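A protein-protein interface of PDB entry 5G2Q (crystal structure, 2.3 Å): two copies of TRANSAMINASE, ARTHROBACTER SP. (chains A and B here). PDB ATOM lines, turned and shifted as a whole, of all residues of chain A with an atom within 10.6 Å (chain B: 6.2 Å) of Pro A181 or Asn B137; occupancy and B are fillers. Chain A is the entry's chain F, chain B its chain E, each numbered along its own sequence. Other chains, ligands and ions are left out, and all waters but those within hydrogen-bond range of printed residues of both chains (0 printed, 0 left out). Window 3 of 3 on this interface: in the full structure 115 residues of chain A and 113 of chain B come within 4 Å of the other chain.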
ATOM      1  N   GLY A 153      31.515   6.408  20.354  1.00  0.00           N
ATOM      2  CA  GLY A 153      32.695   6.431  21.236  1.00  0.00           C
ATOM      3  C   GLY A 153      34.082   6.528  20.618  1.00  0.00           C
ATOM      4  O   GLY A 153      34.723   7.550  20.709  1.00  0.00           O
ATOM      5  N   ARG A 165      31.224  16.916  17.102  1.00  0.00           N
ATOM      6  CA  ARG A 165      31.594  15.966  18.165  1.00  0.00           C
ATOM      7  C   ARG A 165      30.466  15.747  19.200  1.00  0.00           C
ATOM      8  O   ARG A 165      30.697  15.335  20.334  1.00  0.00           O
ATOM      9  CB  ARG A 165      32.897  16.436  18.836  1.00  0.00           C
ATOM     10  CG  ARG A 165      34.142  16.085  18.029  1.00  0.00           C
ATOM     11  CD  ARG A 165      34.387  14.575  18.024  1.00  0.00           C
ATOM     12  NE  ARG A 165      34.616  14.100  19.387  1.00  0.00           N
ATOM     13  CZ  ARG A 165      35.796  14.114  19.993  1.00  0.00           C
ATOM     14  NH1 ARG A 165      36.875  14.515  19.342  1.00  0.00           N
ATOM     15  NH2 ARG A 165      35.892  13.706  21.248  1.00  0.00           N
ATOM     16  N   SER A 166      29.241  16.035  18.773  1.00  0.00           N
ATOM     17  CA  SER A 166      28.016  15.825  19.557  1.00  0.00           C
ATOM     18  C   SER A 166      27.849  16.731  20.777  1.00  0.00           C
ATOM     19  O   SER A 166      27.145  16.384  21.730  1.00  0.00           O
ATOM     20  CB  SER A 166      27.821  14.341  19.908  1.00  0.00           C
ATOM     21  OG  SER A 166      27.962  13.591  18.724  1.00  0.00           O
ATOM     22  N   GLY A 167      28.437  17.921  20.710  1.00  0.00           N
ATOM     23  CA  GLY A 167      28.213  18.904  21.744  1.00  0.00           C
ATOM     24  C   GLY A 167      26.944  19.710  21.584  1.00  0.00           C
ATOM     25  O   GLY A 167      26.117  19.428  20.716  1.00  0.00           O
ATOM     26  N   LEU A 168      26.802  20.716  22.449  1.00  0.00           N
ATOM     27  CA  LEU A 168      25.672  21.651  22.454  1.00  0.00           C
ATOM     28  C   LEU A 168      26.138  23.120  22.325  1.00  0.00           C
ATOM     29  O   LEU A 168      27.077  23.570  23.034  1.00  0.00           O
ATOM     30  CB  LEU A 168      24.846  21.482  23.737  1.00  0.00           C
ATOM     31  CG  LEU A 168      24.308  20.081  24.032  1.00  0.00           C
ATOM     32  CD1 LEU A 168      23.681  20.076  25.408  1.00  0.00           C
ATOM     33  CD2 LEU A 168      23.288  19.697  22.973  1.00  0.00           C
ATOM     34  N   SER A 175      27.424  30.841  24.319  1.00  0.00           N
ATOM     35  CA  SER A 175      27.589  30.949  25.773  1.00  0.00           C
ATOM     36  C   SER A 175      27.009  29.744  26.532  1.00  0.00           C
ATOM     37  O   SER A 175      27.401  29.435  27.658  1.00  0.00           O
ATOM     38  CB  SER A 175      26.935  32.232  26.255  1.00  0.00           C
ATOM     39  OG  SER A 175      27.576  33.348  25.672  1.00  0.00           O
ATOM     40  N   PHE A 176      26.045  29.101  25.889  1.00  0.00           N
ATOM     41  CA  PHE A 176      25.466  27.818  26.297  1.00  0.00           C
ATOM     42  C   PHE A 176      26.465  26.660  26.035  1.00  0.00           C
ATOM     43  O   PHE A 176      26.112  25.479  26.111  1.00  0.00           O
ATOM     44  CB  PHE A 176      24.243  27.576  25.370  1.00  0.00           C
ATOM     45  CG  PHE A 176      22.891  27.977  25.950  1.00  0.00           C
ATOM     46  CD1 PHE A 176      22.775  28.725  27.127  1.00  0.00           C
ATOM     47  CD2 PHE A 176      21.714  27.603  25.286  1.00  0.00           C
ATOM     48  CE1 PHE A 176      21.518  29.067  27.629  1.00  0.00           C
ATOM     49  CE2 PHE A 176      20.465  27.946  25.788  1.00  0.00           C
ATOM     50  CZ  PHE A 176      20.366  28.683  26.958  1.00  0.00           C
ATOM     51  N   SER A 177      27.705  26.996  25.697  1.00  0.00           N
ATOM     52  CA  SER A 177      28.430  26.144  24.758  1.00  0.00           C
ATOM     53  C   SER A 177      29.275  25.106  25.440  1.00  0.00           C
ATOM     54  O   SER A 177      30.099  25.423  26.281  1.00  0.00           O
ATOM     55  CB  SER A 177      29.247  27.004  23.791  1.00  0.00           C
ATOM     56  OG  SER A 177      30.332  26.288  23.238  1.00  0.00           O
ATOM     57  N   ALA A 178      29.081  23.852  25.060  1.00  0.00           N
ATOM     58  CA  ALA A 178      29.715  22.781  25.812  1.00  0.00           C
ATOM     59  C   ALA A 178      30.046  21.597  24.924  1.00  0.00           C
ATOM     60  O   ALA A 178      29.300  21.325  23.972  1.00  0.00           O
ATOM     61  CB  ALA A 178      28.816  22.367  26.966  1.00  0.00           C
ATOM     62  N   GLN A 179      31.176  20.931  25.200  1.00  0.00           N
ATOM     63  CA  GLN A 179      31.468  19.619  24.591  1.00  0.00           C
ATOM     64  C   GLN A 179      31.117  18.525  25.610  1.00  0.00           C
ATOM     65  O   GLN A 179      30.861  18.829  26.755  1.00  0.00           O
ATOM     66  CB  GLN A 179      32.902  19.483  24.052  1.00  0.00           C
ATOM     67  CG  GLN A 179      33.340  20.536  23.022  1.00  0.00           C
ATOM     68  CD  GLN A 179      32.774  20.333  21.614  1.00  0.00           C
ATOM     69  OE1 GLN A 179      31.872  19.541  21.380  1.00  0.00           O
ATOM     70  NE2 GLN A 179      33.308  21.073  20.671  1.00  0.00           N
ATOM     71  N   ILE A 180      31.063  17.266  25.196  1.00  0.00           N
ATOM     72  CA  ILE A 180      30.707  16.195  26.136  1.00  0.00           C
ATOM     73  C   ILE A 180      31.817  16.042  27.180  1.00  0.00           C
ATOM     74  O   ILE A 180      32.982  15.871  26.821  1.00  0.00           O
ATOM     75  CB  ILE A 180      30.527  14.832  25.449  1.00  0.00           C
ATOM     76  CG1 ILE A 180      29.458  14.876  24.374  1.00  0.00           C
ATOM     77  CG2 ILE A 180      30.229  13.745  26.483  1.00  0.00           C
ATOM     78  CD1 ILE A 180      29.707  13.778  23.384  1.00  0.00           C
ATOM     79  N   PRO A 181      31.465  16.119  28.466  1.00  0.00           N
ATOM     80  CA  PRO A 181      32.503  15.995  29.539  1.00  0.00           C
ATOM     81  C   PRO A 181      33.282  14.672  29.403  1.00  0.00           C
ATOM     82  O   PRO A 181      32.671  13.640  29.093  1.00  0.00           O
ATOM     83  CB  PRO A 181      31.682  16.025  30.826  1.00  0.00           C
ATOM     84  CG  PRO A 181      30.404  16.727  30.446  1.00  0.00           C
ATOM     85  CD  PRO A 181      30.123  16.400  29.002  1.00  0.00           C
ATOM     86  N   GLY A 182      34.607  14.706  29.576  1.00  0.00           N
ATOM     87  CA  GLY A 182      35.460  13.548  29.268  1.00  0.00           C
ATOM     88  C   GLY A 182      36.087  13.622  27.879  1.00  0.00           C
ATOM     89  O   GLY A 182      37.305  13.710  27.716  1.00  0.00           O
ATOM     90  N   SER A 183      35.245  13.569  26.864  1.00  0.00           N
ATOM     91  CA  SER A 183      35.675  13.762  25.495  1.00  0.00           C
ATOM     92  C   SER A 183      36.000  15.253  25.259  1.00  0.00           C
ATOM     93  O   SER A 183      37.110  15.630  24.847  1.00  0.00           O
ATOM     94  CB  SER A 183      34.543  13.330  24.564  1.00  0.00           C
ATOM     95  OG  SER A 183      33.428  14.199  24.703  1.00  0.00           O
ATOM     96  N   SER A 187      42.561  10.757  23.557  1.00  0.00           N
ATOM     97  CA  SER A 187      42.454   9.547  24.380  1.00  0.00           C
ATOM     98  C   SER A 187      42.969   8.334  23.597  1.00  0.00           C
ATOM     99  O   SER A 187      42.178   7.529  23.076  1.00  0.00           O
ATOM    100  CB  SER A 187      41.003   9.320  24.812  1.00  0.00           C
ATOM    101  OG  SER A 187      40.876   8.099  25.539  1.00  0.00           O
ATOM    102  N   ARG A 409      31.680  26.373  15.146  1.00  0.00           N
ATOM    103  CA  ARG A 409      30.589  25.516  15.656  1.00  0.00           C
ATOM    104  C   ARG A 409      29.215  26.151  15.326  1.00  0.00           C
ATOM    105  O   ARG A 409      29.150  27.258  14.796  1.00  0.00           O
ATOM    106  CB  ARG A 409      30.735  25.301  17.162  1.00  0.00           C
ATOM    107  CG  ARG A 409      32.026  24.610  17.614  1.00  0.00           C
ATOM    108  CD  ARG A 409      32.014  24.404  19.115  1.00  0.00           C
ATOM    109  NE  ARG A 409      31.025  23.398  19.534  1.00  0.00           N
ATOM    110  CZ  ARG A 409      30.584  23.286  20.786  1.00  0.00           C
ATOM    111  NH1 ARG A 409      31.032  24.123  21.712  1.00  0.00           N
ATOM    112  NH2 ARG A 409      29.680  22.347  21.118  1.00  0.00           N
ATOM    113  N   ASN B 130      26.207  10.129  26.214  1.00  0.00           N
ATOM    114  CA  ASN B 130      26.373  11.486  25.736  1.00  0.00           C
ATOM    115  C   ASN B 130      25.354  12.466  26.344  1.00  0.00           C
ATOM    116  O   ASN B 130      25.750  13.534  26.846  1.00  0.00           O
ATOM    117  CB  ASN B 130      26.328  11.512  24.204  1.00  0.00           C
ATOM    118  CG  ASN B 130      27.537  10.833  23.577  1.00  0.00           C
ATOM    119  OD1 ASN B 130      28.440  10.377  24.282  1.00  0.00           O
ATOM    120  ND2 ASN B 130      27.568  10.776  22.250  1.00  0.00           N
ATOM    121  N   ALA B 132      23.354  11.989  29.144  1.00  0.00           N
ATOM    122  CA  ALA B 132      23.546  12.054  30.601  1.00  0.00           C
ATOM    123  C   ALA B 132      24.731  12.996  31.024  1.00  0.00           C
ATOM    124  O   ALA B 132      24.581  13.828  31.917  1.00  0.00           O
ATOM    125  CB  ALA B 132      23.712  10.658  31.174  1.00  0.00           C
ATOM    126  N   ARG B 133      25.878  12.882  30.360  1.00  0.00           N
ATOM    127  CA  ARG B 133      27.028  13.723  30.676  1.00  0.00           C
ATOM    128  C   ARG B 133      26.783  15.198  30.307  1.00  0.00           C
ATOM    129  O   ARG B 133      27.123  16.070  31.079  1.00  0.00           O
ATOM    130  CB  ARG B 133      28.269  13.204  29.977  1.00  0.00           C
ATOM    131  CG  ARG B 133      28.691  11.824  30.421  1.00  0.00           C
ATOM    132  CD  ARG B 133      29.767  11.274  29.522  1.00  0.00           C
ATOM    133  NE  ARG B 133      30.588  10.376  30.297  1.00  0.00           N
ATOM    134  CZ  ARG B 133      30.908   9.120  29.989  1.00  0.00           C
ATOM    135  NH1 ARG B 133      30.503   8.572  28.840  1.00  0.00           N
ATOM    136  NH2 ARG B 133      31.656   8.415  30.862  1.00  0.00           N
ATOM    137  N   LEU B 134      26.138  15.458  29.155  1.00  0.00           N
ATOM    138  CA  LEU B 134      25.717  16.809  28.805  1.00  0.00           C
ATOM    139  C   LEU B 134      24.706  17.435  29.746  1.00  0.00           C
ATOM    140  O   LEU B 134      24.874  18.576  30.154  1.00  0.00           O
ATOM    141  CB  LEU B 134      25.169  16.865  27.386  1.00  0.00           C
ATOM    142  CG  LEU B 134      26.178  16.744  26.258  1.00  0.00           C
ATOM    143  CD1 LEU B 134      25.488  16.318  24.970  1.00  0.00           C
ATOM    144  CD2 LEU B 134      26.924  18.058  26.119  1.00  0.00           C
ATOM    145  N   TYR B 135      23.647  16.714  30.078  1.00  0.00           N
ATOM    146  CA  TYR B 135      22.636  17.233  31.001  1.00  0.00           C
ATOM    147  C   TYR B 135      23.219  17.580  32.394  1.00  0.00           C
ATOM    148  O   TYR B 135      22.904  18.649  32.962  1.00  0.00           O
ATOM    149  CB  TYR B 135      21.481  16.227  31.119  1.00  0.00           C
ATOM    150  CG  TYR B 135      20.391  16.639  32.074  1.00  0.00           C
ATOM    151  CD1 TYR B 135      19.530  17.702  31.776  1.00  0.00           C
ATOM    152  CD2 TYR B 135      20.221  15.970  33.280  1.00  0.00           C
ATOM    153  CE1 TYR B 135      18.531  18.082  32.664  1.00  0.00           C
ATOM    154  CE2 TYR B 135      19.229  16.331  34.164  1.00  0.00           C
ATOM    155  CZ  TYR B 135      18.399  17.384  33.862  1.00  0.00           C
ATOM    156  OH  TYR B 135      17.423  17.713  34.762  1.00  0.00           O
ATOM    157  N   THR B 136      24.056  16.697  32.943  1.00  0.00           N
ATOM    158  CA  THR B 136      24.594  16.916  34.294  1.00  0.00           C
ATOM    159  C   THR B 136      25.870  17.756  34.270  1.00  0.00           C
ATOM    160  O   THR B 136      26.296  18.294  35.294  1.00  0.00           O
ATOM    161  CB  THR B 136      24.907  15.584  35.016  1.00  0.00           C
ATOM    162  OG1 THR B 136      25.863  14.855  34.248  1.00  0.00           O
ATOM    163  CG2 THR B 136      23.707  14.738  35.141  1.00  0.00           C
ATOM    164  N   ASN B 137      26.471  17.870  33.090  1.00  0.00           N
ATOM    165  CA  ASN B 137      27.811  18.452  32.916  1.00  0.00           C
ATOM    166  C   ASN B 137      28.825  17.760  33.825  1.00  0.00           C
ATOM    167  O   ASN B 137      29.685  18.412  34.400  1.00  0.00           O
ATOM    168  CB  ASN B 137      27.820  19.963  33.157  1.00  0.00           C
ATOM    169  CG  ASN B 137      29.033  20.661  32.519  1.00  0.00           C
ATOM    170  OD1 ASN B 137      29.520  20.254  31.474  1.00  0.00           O
ATOM    171  ND2 ASN B 137      29.521  21.717  33.166  1.00  0.00           N
ATOM    172  N   ARG B 138      28.707  16.437  33.931  1.00  0.00           N
ATOM    173  CA  ARG B 138      29.613  15.610  34.718  1.00  0.00           C
ATOM    174  C   ARG B 138      30.255  14.513  33.875  1.00  0.00           C
ATOM    175  O   ARG B 138      29.657  14.011  32.932  1.00  0.00           O
ATOM    176  CB  ARG B 138      28.856  14.994  35.882  1.00  0.00           C
ATOM    177  CG  ARG B 138      28.202  16.029  36.778  1.00  0.00           C
ATOM    178  CD  ARG B 138      27.400  15.336  37.839  1.00  0.00           C
ATOM    179  NE  ARG B 138      26.534  16.253  38.550  1.00  0.00           N
ATOM    180  CZ  ARG B 138      25.543  15.840  39.319  1.00  0.00           C
ATOM    181  NH1 ARG B 138      25.321  14.534  39.440  1.00  0.00           N
ATOM    182  NH2 ARG B 138      24.771  16.712  39.949  1.00  0.00           N
ATOM    183  N   PRO B 139      31.482  14.129  34.205  1.00  0.00           N
ATOM    184  CA  PRO B 139      32.194  13.162  33.387  1.00  0.00           C
ATOM    185  C   PRO B 139      31.913  11.658  33.656  1.00  0.00           C
ATOM    186  O   PRO B 139      31.852  10.863  32.700  1.00  0.00           O
ATOM    187  CB  PRO B 139      33.649  13.479  33.702  1.00  0.00           C
ATOM    188  CG  PRO B 139      33.608  13.939  35.121  1.00  0.00           C
ATOM    189  CD  PRO B 139      32.360  14.780  35.185  1.00  0.00           C
ATOM    190  N   ALA B 188      36.881   7.343  32.676  1.00  0.00           N
ATOM    191  CA  ALA B 188      35.647   8.085  32.969  1.00  0.00           C
ATOM    192  C   ALA B 188      34.475   7.163  33.356  1.00  0.00           C
ATOM    193  O   ALA B 188      33.299   7.557  33.279  1.00  0.00           O
ATOM    194  CB  ALA B 188      35.273   8.988  31.799  1.00  0.00           C
ATOM    195  N   GLU B 229      28.950  15.263  42.628  1.00  0.00           N
ATOM    196  CA  GLU B 229      29.099  16.327  41.649  1.00  0.00           C
ATOM    197  C   GLU B 229      29.959  15.920  40.422  1.00  0.00           C
ATOM    198  O   GLU B 229      29.985  16.647  39.407  1.00  0.00           O
ATOM    199  CB  GLU B 229      29.604  17.617  42.327  1.00  0.00           C
ATOM    200  CG  GLU B 229      31.111  17.769  42.399  1.00  0.00           C
ATOM    201  CD  GLU B 229      31.744  17.039  43.567  1.00  0.00           C
ATOM    202  OE1 GLU B 229      31.056  16.249  44.281  1.00  0.00           O
ATOM    203  OE2 GLU B 229      32.944  17.287  43.793  1.00  0.00           O
ATOM    204  N   ALA B 232      27.729  11.645  36.526  1.00  0.00           N
ATOM    205  CA  ALA B 232      26.567  11.909  35.634  1.00  0.00           C
ATOM    206  C   ALA B 232      25.411  10.946  35.869  1.00  0.00           C
ATOM    207  O   ALA B 232      24.254  11.370  35.996  1.00  0.00           O
ATOM    208  CB  ALA B 232      26.994  11.842  34.183  1.00  0.00           C
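Printed residues of chain B that touch a printed residue of chain A: Asn B130, Arg B133, Leu B134, Asn B137, Arg B138 and Pro B139. Of the 16 printed residues of chain A, 4 touch a printed residue of chain B.
O of Ala B188 sits at hydrogen-bond distance from NH2 of Arg B133, at 3.0 Å. The backbone carbonyl oxygen of Pro B139 sits at hydrogen-bond distance from the guanidinium group of Arg B133, 2.8 Å away. OG1 of Thr B136 lies close to N of Arg B138 (3.3 Å). The backbone carbonyl oxygen (O) of Ile A180 lies within hydrogen-bond range of the side-chain hydroxyl (OG) of Ser A183 (2.7 Å). The backbone carbonyl oxygen (O) of Leu A168 sits at hydrogen-bond distance from the backbone NH (N) of Ala A178, at 2.9 Å. N of Arg B138 is in hydrogen-bond range of O of Arg B133 (3.3 Å).
No position is printed for both chains.
Of chain B, only Arg B133 (3.4 Å), Asn B137 (3.8 Å), Arg B138 (3.5 Å) and Pro B139 (3.9 Å) come within 4 Å of Pro A181. Asn B137 touches just one residue of chain A: Pro A181 (3.8 Å). Of chain A, only Ile A180 (3.9 Å) and Pro A181 (3.4 Å) come within 4 Å of Arg B133. Leu B134 touches just these residues of chain A: Ser A166 (3.6 Å) and Leu A168 (3.9 Å). No residue of chain A comes within 4 Å of Thr B136. Pro B139 touches just one residue of chain A: Pro A181. Of the printed residues of chain A, Arg B138 touches Pro A181 (3.5 Å). Printed residues of chain B within 4 Å of Ser A166: Leu B134 (3.6 Å). The nearest residue of chain A that does not touch Asn B137 is Ala A178 (5.0 Å).
Among the printed residues, pairs that only touch across the chains: Ser A166 with Leu B134 (3.6 Å), Leu A168 with Leu B134 (3.9 Å), Ile A180 with Asn B130 (3.7 Å), Ile A180 with Arg B133 (3.9 Å), Pro A181 with Arg B133 (3.4 Å), Pro A181 with Asn B137 (3.8 Å), Pro A181 with Arg B138 (3.5 Å) and Pro A181 with Pro B139 (3.9 Å).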
